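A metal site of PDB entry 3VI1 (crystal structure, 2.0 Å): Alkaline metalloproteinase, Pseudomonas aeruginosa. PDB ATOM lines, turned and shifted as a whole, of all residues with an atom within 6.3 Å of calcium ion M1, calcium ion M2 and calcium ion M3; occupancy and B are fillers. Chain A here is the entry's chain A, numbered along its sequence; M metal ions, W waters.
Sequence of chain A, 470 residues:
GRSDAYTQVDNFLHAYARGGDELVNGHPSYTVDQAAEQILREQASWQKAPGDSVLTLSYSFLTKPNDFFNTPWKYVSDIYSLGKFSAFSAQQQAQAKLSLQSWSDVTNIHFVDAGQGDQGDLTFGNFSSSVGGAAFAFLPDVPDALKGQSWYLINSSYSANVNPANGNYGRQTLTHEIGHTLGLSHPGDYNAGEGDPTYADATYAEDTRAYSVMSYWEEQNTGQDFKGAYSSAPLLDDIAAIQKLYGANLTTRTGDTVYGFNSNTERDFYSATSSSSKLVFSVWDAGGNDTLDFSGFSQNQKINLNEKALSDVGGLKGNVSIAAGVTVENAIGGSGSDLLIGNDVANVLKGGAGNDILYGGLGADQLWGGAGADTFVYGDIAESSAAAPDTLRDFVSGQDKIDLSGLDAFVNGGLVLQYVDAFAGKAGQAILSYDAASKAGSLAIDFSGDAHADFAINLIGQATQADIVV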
ATOM      1  N   GLY A 333      10.815  21.011 -19.355  1.00  0.00           N
ATOM      2  CA  GLY A 333       9.380  20.779 -19.207  1.00  0.00           C
ATOM      3  C   GLY A 333       8.843  21.345 -17.898  1.00  0.00           C
ATOM      4  O   GLY A 333       9.615  21.816 -17.062  1.00  0.00           O
ATOM      5  N   GLY A 334       7.532  21.297 -17.736  1.00  0.00           N
ATOM      6  CA  GLY A 334       6.889  21.774 -16.508  1.00  0.00           C
ATOM      7  C   GLY A 334       6.613  20.649 -15.526  1.00  0.00           C
ATOM      8  O   GLY A 334       7.221  19.587 -15.602  1.00  0.00           O
ATOM      9  N   SER A 335       5.677  20.891 -14.607  1.00  0.00           N
ATOM     10  CA  SER A 335       5.327  19.917 -13.570  1.00  0.00           C
ATOM     11  C   SER A 335       4.420  18.781 -14.069  1.00  0.00           C
ATOM     12  O   SER A 335       4.233  17.782 -13.374  1.00  0.00           O
ATOM     13  CB  SER A 335       4.704  20.607 -12.357  1.00  0.00           C
ATOM     14  OG  SER A 335       3.548  21.337 -12.723  1.00  0.00           O
ATOM     15  N   GLY A 336       3.870  18.941 -15.276  1.00  0.00           N
ATOM     16  CA  GLY A 336       3.031  17.920 -15.888  1.00  0.00           C
ATOM     17  C   GLY A 336       3.830  16.821 -16.547  1.00  0.00           C
ATOM     18  O   GLY A 336       5.065  16.884 -16.614  1.00  0.00           O
ATOM     19  N   SER A 337       3.130  15.794 -17.028  1.00  0.00           N
ATOM     20  CA  SER A 337       3.769  14.694 -17.742  1.00  0.00           C
ATOM     21  C   SER A 337       4.088  15.099 -19.177  1.00  0.00           C
ATOM     22  O   SER A 337       3.209  15.171 -20.023  1.00  0.00           O
ATOM     23  CB  SER A 337       2.876  13.444 -17.703  1.00  0.00           C
ATOM     24  OG  SER A 337       2.786  12.935 -16.392  1.00  0.00           O
ATOM     25  N   ASP A 338       5.369  15.368 -19.426  1.00  0.00           N
ATOM     26  CA  ASP A 338       5.795  15.988 -20.677  1.00  0.00           C
ATOM     27  C   ASP A 338       6.481  15.033 -21.646  1.00  0.00           C
ATOM     28  O   ASP A 338       6.987  13.975 -21.260  1.00  0.00           O
ATOM     29  CB  ASP A 338       6.731  17.173 -20.398  1.00  0.00           C
ATOM     30  CG  ASP A 338       6.107  18.204 -19.475  1.00  0.00           C
ATOM     31  OD1 ASP A 338       4.936  18.587 -19.700  1.00  0.00           O
ATOM     32  OD2 ASP A 338       6.800  18.634 -18.523  1.00  0.00           O
ATOM     33  N   LEU A 340       9.558  15.306 -24.371  1.00  0.00           N
ATOM     34  CA  LEU A 340      10.672  16.137 -24.813  1.00  0.00           C
ATOM     35  C   LEU A 340      11.503  15.451 -25.893  1.00  0.00           C
ATOM     36  O   LEU A 340      12.195  14.458 -25.625  1.00  0.00           O
ATOM     37  CB  LEU A 340      11.565  16.546 -23.622  1.00  0.00           C
ATOM     38  CG  LEU A 340      11.141  17.746 -22.780  1.00  0.00           C
ATOM     39  CD1 LEU A 340      10.091  17.357 -21.750  1.00  0.00           C
ATOM     40  CD2 LEU A 340      12.352  18.350 -22.088  1.00  0.00           C
ATOM     41  N   LYS A 350      15.396  18.497 -19.667  1.00  0.00           N
ATOM     42  CA  LYS A 350      14.953  18.393 -18.280  1.00  0.00           C
ATOM     43  C   LYS A 350      13.437  18.242 -18.201  1.00  0.00           C
ATOM     44  O   LYS A 350      12.688  19.109 -18.662  1.00  0.00           O
ATOM     45  CB  LYS A 350      15.438  19.606 -17.467  1.00  0.00           C
ATOM     46  CG  LYS A 350      16.949  19.680 -17.324  1.00  0.00           C
ATOM     47  CD  LYS A 350      17.386  20.777 -16.376  1.00  0.00           C
ATOM     48  CE  LYS A 350      18.892  20.741 -16.180  1.00  0.00           C
ATOM     49  NZ  LYS A 350      19.381  21.839 -15.303  1.00  0.00           N
ATOM     50  N   GLY A 351      12.997  17.129 -17.632  1.00  0.00           N
ATOM     51  CA  GLY A 351      11.575  16.809 -17.547  1.00  0.00           C
ATOM     52  C   GLY A 351      10.853  17.501 -16.407  1.00  0.00           C
ATOM     53  O   GLY A 351       9.675  17.852 -16.546  1.00  0.00           O
ATOM     54  N   GLY A 352      11.537  17.691 -15.290  1.00  0.00           N
ATOM     55  CA  GLY A 352      10.922  18.261 -14.084  1.00  0.00           C
ATOM     56  C   GLY A 352      10.020  17.247 -13.407  1.00  0.00           C
ATOM     57  O   GLY A 352      10.235  16.044 -13.515  1.00  0.00           O
ATOM     58  N   ALA A 353       8.993  17.743 -12.721  1.00  0.00           N
ATOM     59  CA  ALA A 353       8.009  16.882 -12.065  1.00  0.00           C
ATOM     60  C   ALA A 353       7.128  16.150 -13.089  1.00  0.00           C
ATOM     61  O   ALA A 353       7.092  16.523 -14.262  1.00  0.00           O
ATOM     62  CB  ALA A 353       7.143  17.693 -11.098  1.00  0.00           C
ATOM     63  N   GLY A 354       6.426  15.113 -12.623  1.00  0.00           N
ATOM     64  CA  GLY A 354       5.560  14.323 -13.496  1.00  0.00           C
ATOM     65  C   GLY A 354       6.310  13.228 -14.235  1.00  0.00           C
ATOM     66  O   GLY A 354       7.533  13.140 -14.160  1.00  0.00           O
ATOM     67  N   ASN A 355       5.557  12.400 -14.967  1.00  0.00           N
ATOM     68  CA  ASN A 355       6.119  11.273 -15.698  1.00  0.00           C
ATOM     69  C   ASN A 355       6.475  11.637 -17.137  1.00  0.00           C
ATOM     70  O   ASN A 355       5.613  11.666 -18.019  1.00  0.00           O
ATOM     71  CB  ASN A 355       5.157  10.080 -15.654  1.00  0.00           C
ATOM     72  CG  ASN A 355       4.891   9.586 -14.245  1.00  0.00           C
ATOM     73  OD1 ASN A 355       5.757   9.676 -13.365  1.00  0.00           O
ATOM     74  ND2 ASN A 355       3.698   9.059 -14.021  1.00  0.00           N
ATOM     75  N   ASP A 356       7.758  11.892 -17.369  1.00  0.00           N
ATOM     76  CA  ASP A 356       8.214  12.445 -18.636  1.00  0.00           C
ATOM     77  C   ASP A 356       8.858  11.416 -19.558  1.00  0.00           C
ATOM     78  O   ASP A 356       9.480  10.454 -19.103  1.00  0.00           O
ATOM     79  CB  ASP A 356       9.185  13.604 -18.408  1.00  0.00           C
ATOM     80  CG  ASP A 356       8.630  14.643 -17.462  1.00  0.00           C
ATOM     81  OD1 ASP A 356       7.633  15.310 -17.823  1.00  0.00           O
ATOM     82  OD2 ASP A 356       9.186  14.811 -16.357  1.00  0.00           O
ATOM     83  N   TRP A 368      17.879  14.772 -17.980  1.00  0.00           N
ATOM     84  CA  TRP A 368      17.399  14.863 -16.605  1.00  0.00           C
ATOM     85  C   TRP A 368      15.912  14.522 -16.581  1.00  0.00           C
ATOM     86  O   TRP A 368      15.108  15.164 -17.240  1.00  0.00           O
ATOM     87  CB  TRP A 368      17.607  16.283 -16.054  1.00  0.00           C
ATOM     88  CG  TRP A 368      19.020  16.810 -16.186  1.00  0.00           C
ATOM     89  CD1 TRP A 368      19.633  17.238 -17.329  1.00  0.00           C
ATOM     90  CD2 TRP A 368      19.968  17.003 -15.124  1.00  0.00           C
ATOM     91  NE1 TRP A 368      20.911  17.655 -17.055  1.00  0.00           N
ATOM     92  CE2 TRP A 368      21.140  17.526 -15.713  1.00  0.00           C
ATOM     93  CE3 TRP A 368      19.948  16.770 -13.740  1.00  0.00           C
ATOM     94  CZ2 TRP A 368      22.290  17.833 -14.957  1.00  0.00           C
ATOM     95  CZ3 TRP A 368      21.080  17.071 -12.994  1.00  0.00           C
ATOM     96  CH2 TRP A 368      22.231  17.602 -13.609  1.00  0.00           C
ATOM     97  N   GLY A 369      15.577  13.486 -15.819  1.00  0.00           N
ATOM     98  CA  GLY A 369      14.187  13.075 -15.676  1.00  0.00           C
ATOM     99  C   GLY A 369      13.427  13.915 -14.670  1.00  0.00           C
ATOM    100  O   GLY A 369      12.261  14.261 -14.880  1.00  0.00           O
ATOM    101  N   GLY A 370      14.097  14.278 -13.576  1.00  0.00           N
ATOM    102  CA  GLY A 370      13.458  14.952 -12.455  1.00  0.00           C
ATOM    103  C   GLY A 370      12.713  13.943 -11.595  1.00  0.00           C
ATOM    104  O   GLY A 370      13.008  12.738 -11.653  1.00  0.00           O
ATOM    105  N   ALA A 371      11.748  14.417 -10.821  1.00  0.00           N
ATOM    106  CA  ALA A 371      10.904  13.539 -10.008  1.00  0.00           C
ATOM    107  C   ALA A 371       9.936  12.753 -10.890  1.00  0.00           C
ATOM    108  O   ALA A 371       9.664  13.151 -12.026  1.00  0.00           O
ATOM    109  CB  ALA A 371      10.160  14.332  -8.961  1.00  0.00           C
ATOM    110  N   GLY A 372       9.413  11.658 -10.356  1.00  0.00           N
ATOM    111  CA  GLY A 372       8.450  10.816 -11.078  1.00  0.00           C
ATOM    112  C   GLY A 372       9.108   9.748 -11.941  1.00  0.00           C
ATOM    113  O   GLY A 372      10.330   9.707 -12.077  1.00  0.00           O
ATOM    114  N   ALA A 373       8.275   8.884 -12.516  1.00  0.00           N
ATOM    115  CA  ALA A 373       8.735   7.790 -13.374  1.00  0.00           C
ATOM    116  C   ALA A 373       8.972   8.276 -14.793  1.00  0.00           C
ATOM    117  O   ALA A 373       8.030   8.491 -15.559  1.00  0.00           O
ATOM    118  CB  ALA A 373       7.716   6.646 -13.353  1.00  0.00           C
ATOM    119  N   ASP A 374      10.241   8.437 -15.152  1.00  0.00           N
ATOM    120  CA  ASP A 374      10.619   8.977 -16.452  1.00  0.00           C
ATOM    121  C   ASP A 374      11.168   7.909 -17.388  1.00  0.00           C
ATOM    122  O   ASP A 374      11.781   6.942 -16.943  1.00  0.00           O
ATOM    123  CB  ASP A 374      11.624  10.119 -16.280  1.00  0.00           C
ATOM    124  CG  ASP A 374      11.111  11.219 -15.385  1.00  0.00           C
ATOM    125  OD1 ASP A 374      10.178  11.944 -15.786  1.00  0.00           O
ATOM    126  OD2 ASP A 374      11.639  11.368 -14.264  1.00  0.00           O
ATOM    127  N   PHE A 376      13.506   7.180 -20.822  1.00  0.00           N
ATOM    128  CA  PHE A 376      14.524   7.637 -21.751  1.00  0.00           C
ATOM    129  C   PHE A 376      14.523   6.711 -22.966  1.00  0.00           C
ATOM    130  O   PHE A 376      14.920   5.547 -22.871  1.00  0.00           O
ATOM    131  CB  PHE A 376      15.893   7.696 -21.067  1.00  0.00           C
ATOM    132  CG  PHE A 376      15.892   8.479 -19.776  1.00  0.00           C
ATOM    133  CD1 PHE A 376      15.755   7.822 -18.553  1.00  0.00           C
ATOM    134  CD2 PHE A 376      15.996   9.871 -19.791  1.00  0.00           C
ATOM    135  CE1 PHE A 376      15.745   8.544 -17.358  1.00  0.00           C
ATOM    136  CE2 PHE A 376      15.986  10.593 -18.596  1.00  0.00           C
ATOM    137  CZ  PHE A 376      15.859   9.934 -17.381  1.00  0.00           C
ATOM    138  N   ASP A 394      20.167  11.889 -13.551  1.00  0.00           N
ATOM    139  CA  ASP A 394      19.451  11.667 -12.290  1.00  0.00           C
ATOM    140  C   ASP A 394      18.625  10.380 -12.286  1.00  0.00           C
ATOM    141  O   ASP A 394      17.505  10.353 -11.774  1.00  0.00           O
ATOM    142  CB  ASP A 394      18.590  12.895 -11.921  1.00  0.00           C
ATOM    143  CG  ASP A 394      17.556  13.236 -12.998  1.00  0.00           C
ATOM    144  OD1 ASP A 394      17.451  12.515 -14.010  1.00  0.00           O
ATOM    145  OD2 ASP A 394      16.833  14.238 -12.812  1.00  0.00           O
ATOM    146  N   VAL A 396      17.003   7.011 -11.354  1.00  0.00           N
ATOM    147  CA  VAL A 396      16.609   6.318 -10.136  1.00  0.00           C
ATOM    148  C   VAL A 396      16.110   4.919 -10.504  1.00  0.00           C
ATOM    149  O   VAL A 396      15.150   4.767 -11.261  1.00  0.00           O
ATOM    150  CB  VAL A 396      15.491   7.083  -9.366  1.00  0.00           C
ATOM    151  CG1 VAL A 396      15.112   6.341  -8.086  1.00  0.00           C
ATOM    152  CG2 VAL A 396      15.936   8.511  -9.045  1.00  0.00           C
ATOM    153  N   GLN A 399      12.216   3.215 -10.710  1.00  0.00           N
ATOM    154  CA  GLN A 399      11.299   4.309 -11.002  1.00  0.00           C
ATOM    155  C   GLN A 399      11.441   4.757 -12.457  1.00  0.00           C
ATOM    156  O   GLN A 399      10.452   4.800 -13.204  1.00  0.00           O
ATOM    157  CB  GLN A 399      11.532   5.485 -10.056  1.00  0.00           C
ATOM    158  CG  GLN A 399      10.450   6.558 -10.095  1.00  0.00           C
ATOM    159  CD  GLN A 399      10.772   7.769  -9.231  1.00  0.00           C
ATOM    160  OE1 GLN A 399      11.921   8.201  -9.155  1.00  0.00           O
ATOM    161  NE2 GLN A 399       9.748   8.321  -8.598  1.00  0.00           N
ATOM    162  N   ASP A 400      12.667   5.079 -12.858  1.00  0.00           N
ATOM    163  CA  ASP A 400      12.956   5.482 -14.231  1.00  0.00           C
ATOM    164  C   ASP A 400      13.139   4.280 -15.135  1.00  0.00           C
ATOM    165  O   ASP A 400      13.370   3.155 -14.660  1.00  0.00           O
ATOM    166  CB  ASP A 400      14.204   6.367 -14.276  1.00  0.00           C
ATOM    167  CG  ASP A 400      14.030   7.672 -13.528  1.00  0.00           C
ATOM    168  OD1 ASP A 400      12.917   8.254 -13.567  1.00  0.00           O
ATOM    169  OD2 ASP A 400      15.011   8.130 -12.907  1.00  0.00           O
HETATM  170 CA    CA M   1       7.399  17.359 -16.472  1.00  0.00          CA
HETATM  171 CA    CA M   2       9.892  13.840 -14.284  1.00  0.00          CA
HETATM  172 CA    CA M   3      12.649  10.490 -12.364  1.00  0.00          CA
HETATM  173  O   HOH W   1      13.241  10.417 -10.029  1.00  0.00           O
HETATM  174  O   HOH W   2      14.914  10.780 -13.316  1.00  0.00           O
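Water W2 bridges the side-chain carboxylate of Asp 400 and the backbone carbonyl oxygen of Asp 394.
Within 4 Å of calcium ion M2: Gly 352, Ala 353, Gly 354, Asp 356, Gly 369, Gly 370, Ala 371 and Asp 374. The nearest printed residue that does not touch calcium ion M2 is Gly 351 (4.3 Å).
Five residues have an atom within 4 Å of calcium ion M3: Gly 370, Ala 371, Gly 372, Asp 374 and Asp 400.
Calcium ion M2 is bound by the backbone carbonyl oxygen (O) of Gly 352, 2.4 Å away. Calcium ion M2 is bound by O of Ala 371 (2.4 Å). OD2 of Asp 356 is bound to calcium ion M2 (2.4 Å). OD1 of Asp 374 binds calcium ion M2, at 2.4 Å. The backbone carbonyl oxygen (O) of Gly 354 is bound to calcium ion M2, 2.5 Å away. Calcium ion M2 is bound by O of Gly 369, 2.5 Å away. Slightly farther from calcium ion M2 lies OD2 of Asp 374 (3.0 Å).
Six residues have an atom within 4 Å of calcium ion M1: Gly 334, Gly 336, Asp 338, Gly 351, Ala 353 and Asp 356. Along chain A the residues within 4 Å of calcium ion M1 span positions 334 to 356.
O of Gly 351 binds calcium ion M1 (2.3 Å). Calcium ion M1 is bound by O of Ala 353, 2.4 Å away. O of Gly 336 is bound to calcium ion M1, at 2.4 Å. The backbone carbonyl oxygen (O) of Gly 334 is bound to calcium ion M1. The side-chain carboxylate (OD1) of Asp 356 is bound to calcium ion M1 (2.5 Å). OD2 of Asp 338 binds calcium ion M1 (2.5 Å). Calcium ion M1 has six donor atoms within binding distance. Slightly farther from calcium ion M1 lies OD2 of Asp 356 (3.1 Å).
OD2 of Asp 374 binds calcium ion M3 (2.3 Å). Calcium ion M3 is bound by O of Gly 370, 2.4 Å away. Calcium ion M3 is bound by water W1 (2.4 Å). O of Gly 372 is bound to calcium ion M3. Water W2 is bound to calcium ion M3, at 2.5 Å. The side-chain carboxylate (OD1) of Asp 400 binds calcium ion M3, 2.6 Å away. Calcium ion M3 has six donor atoms within binding distance.
The backbone NH (N) of Gly 369 lies within hydrogen-bond range of the side-chain carboxylate (OD1) of Asp 394, at 2.8 Å. The backbone NH of Gly 370 sits at hydrogen-bond distance from the side-chain carboxylate of Asp 394, 2.8 Å away. O of Trp 368 sits at hydrogen-bond distance from N of Gly 351 (2.9 Å). OD2 of Asp 400 is in hydrogen-bond range of N of Val 396 (2.8 Å).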
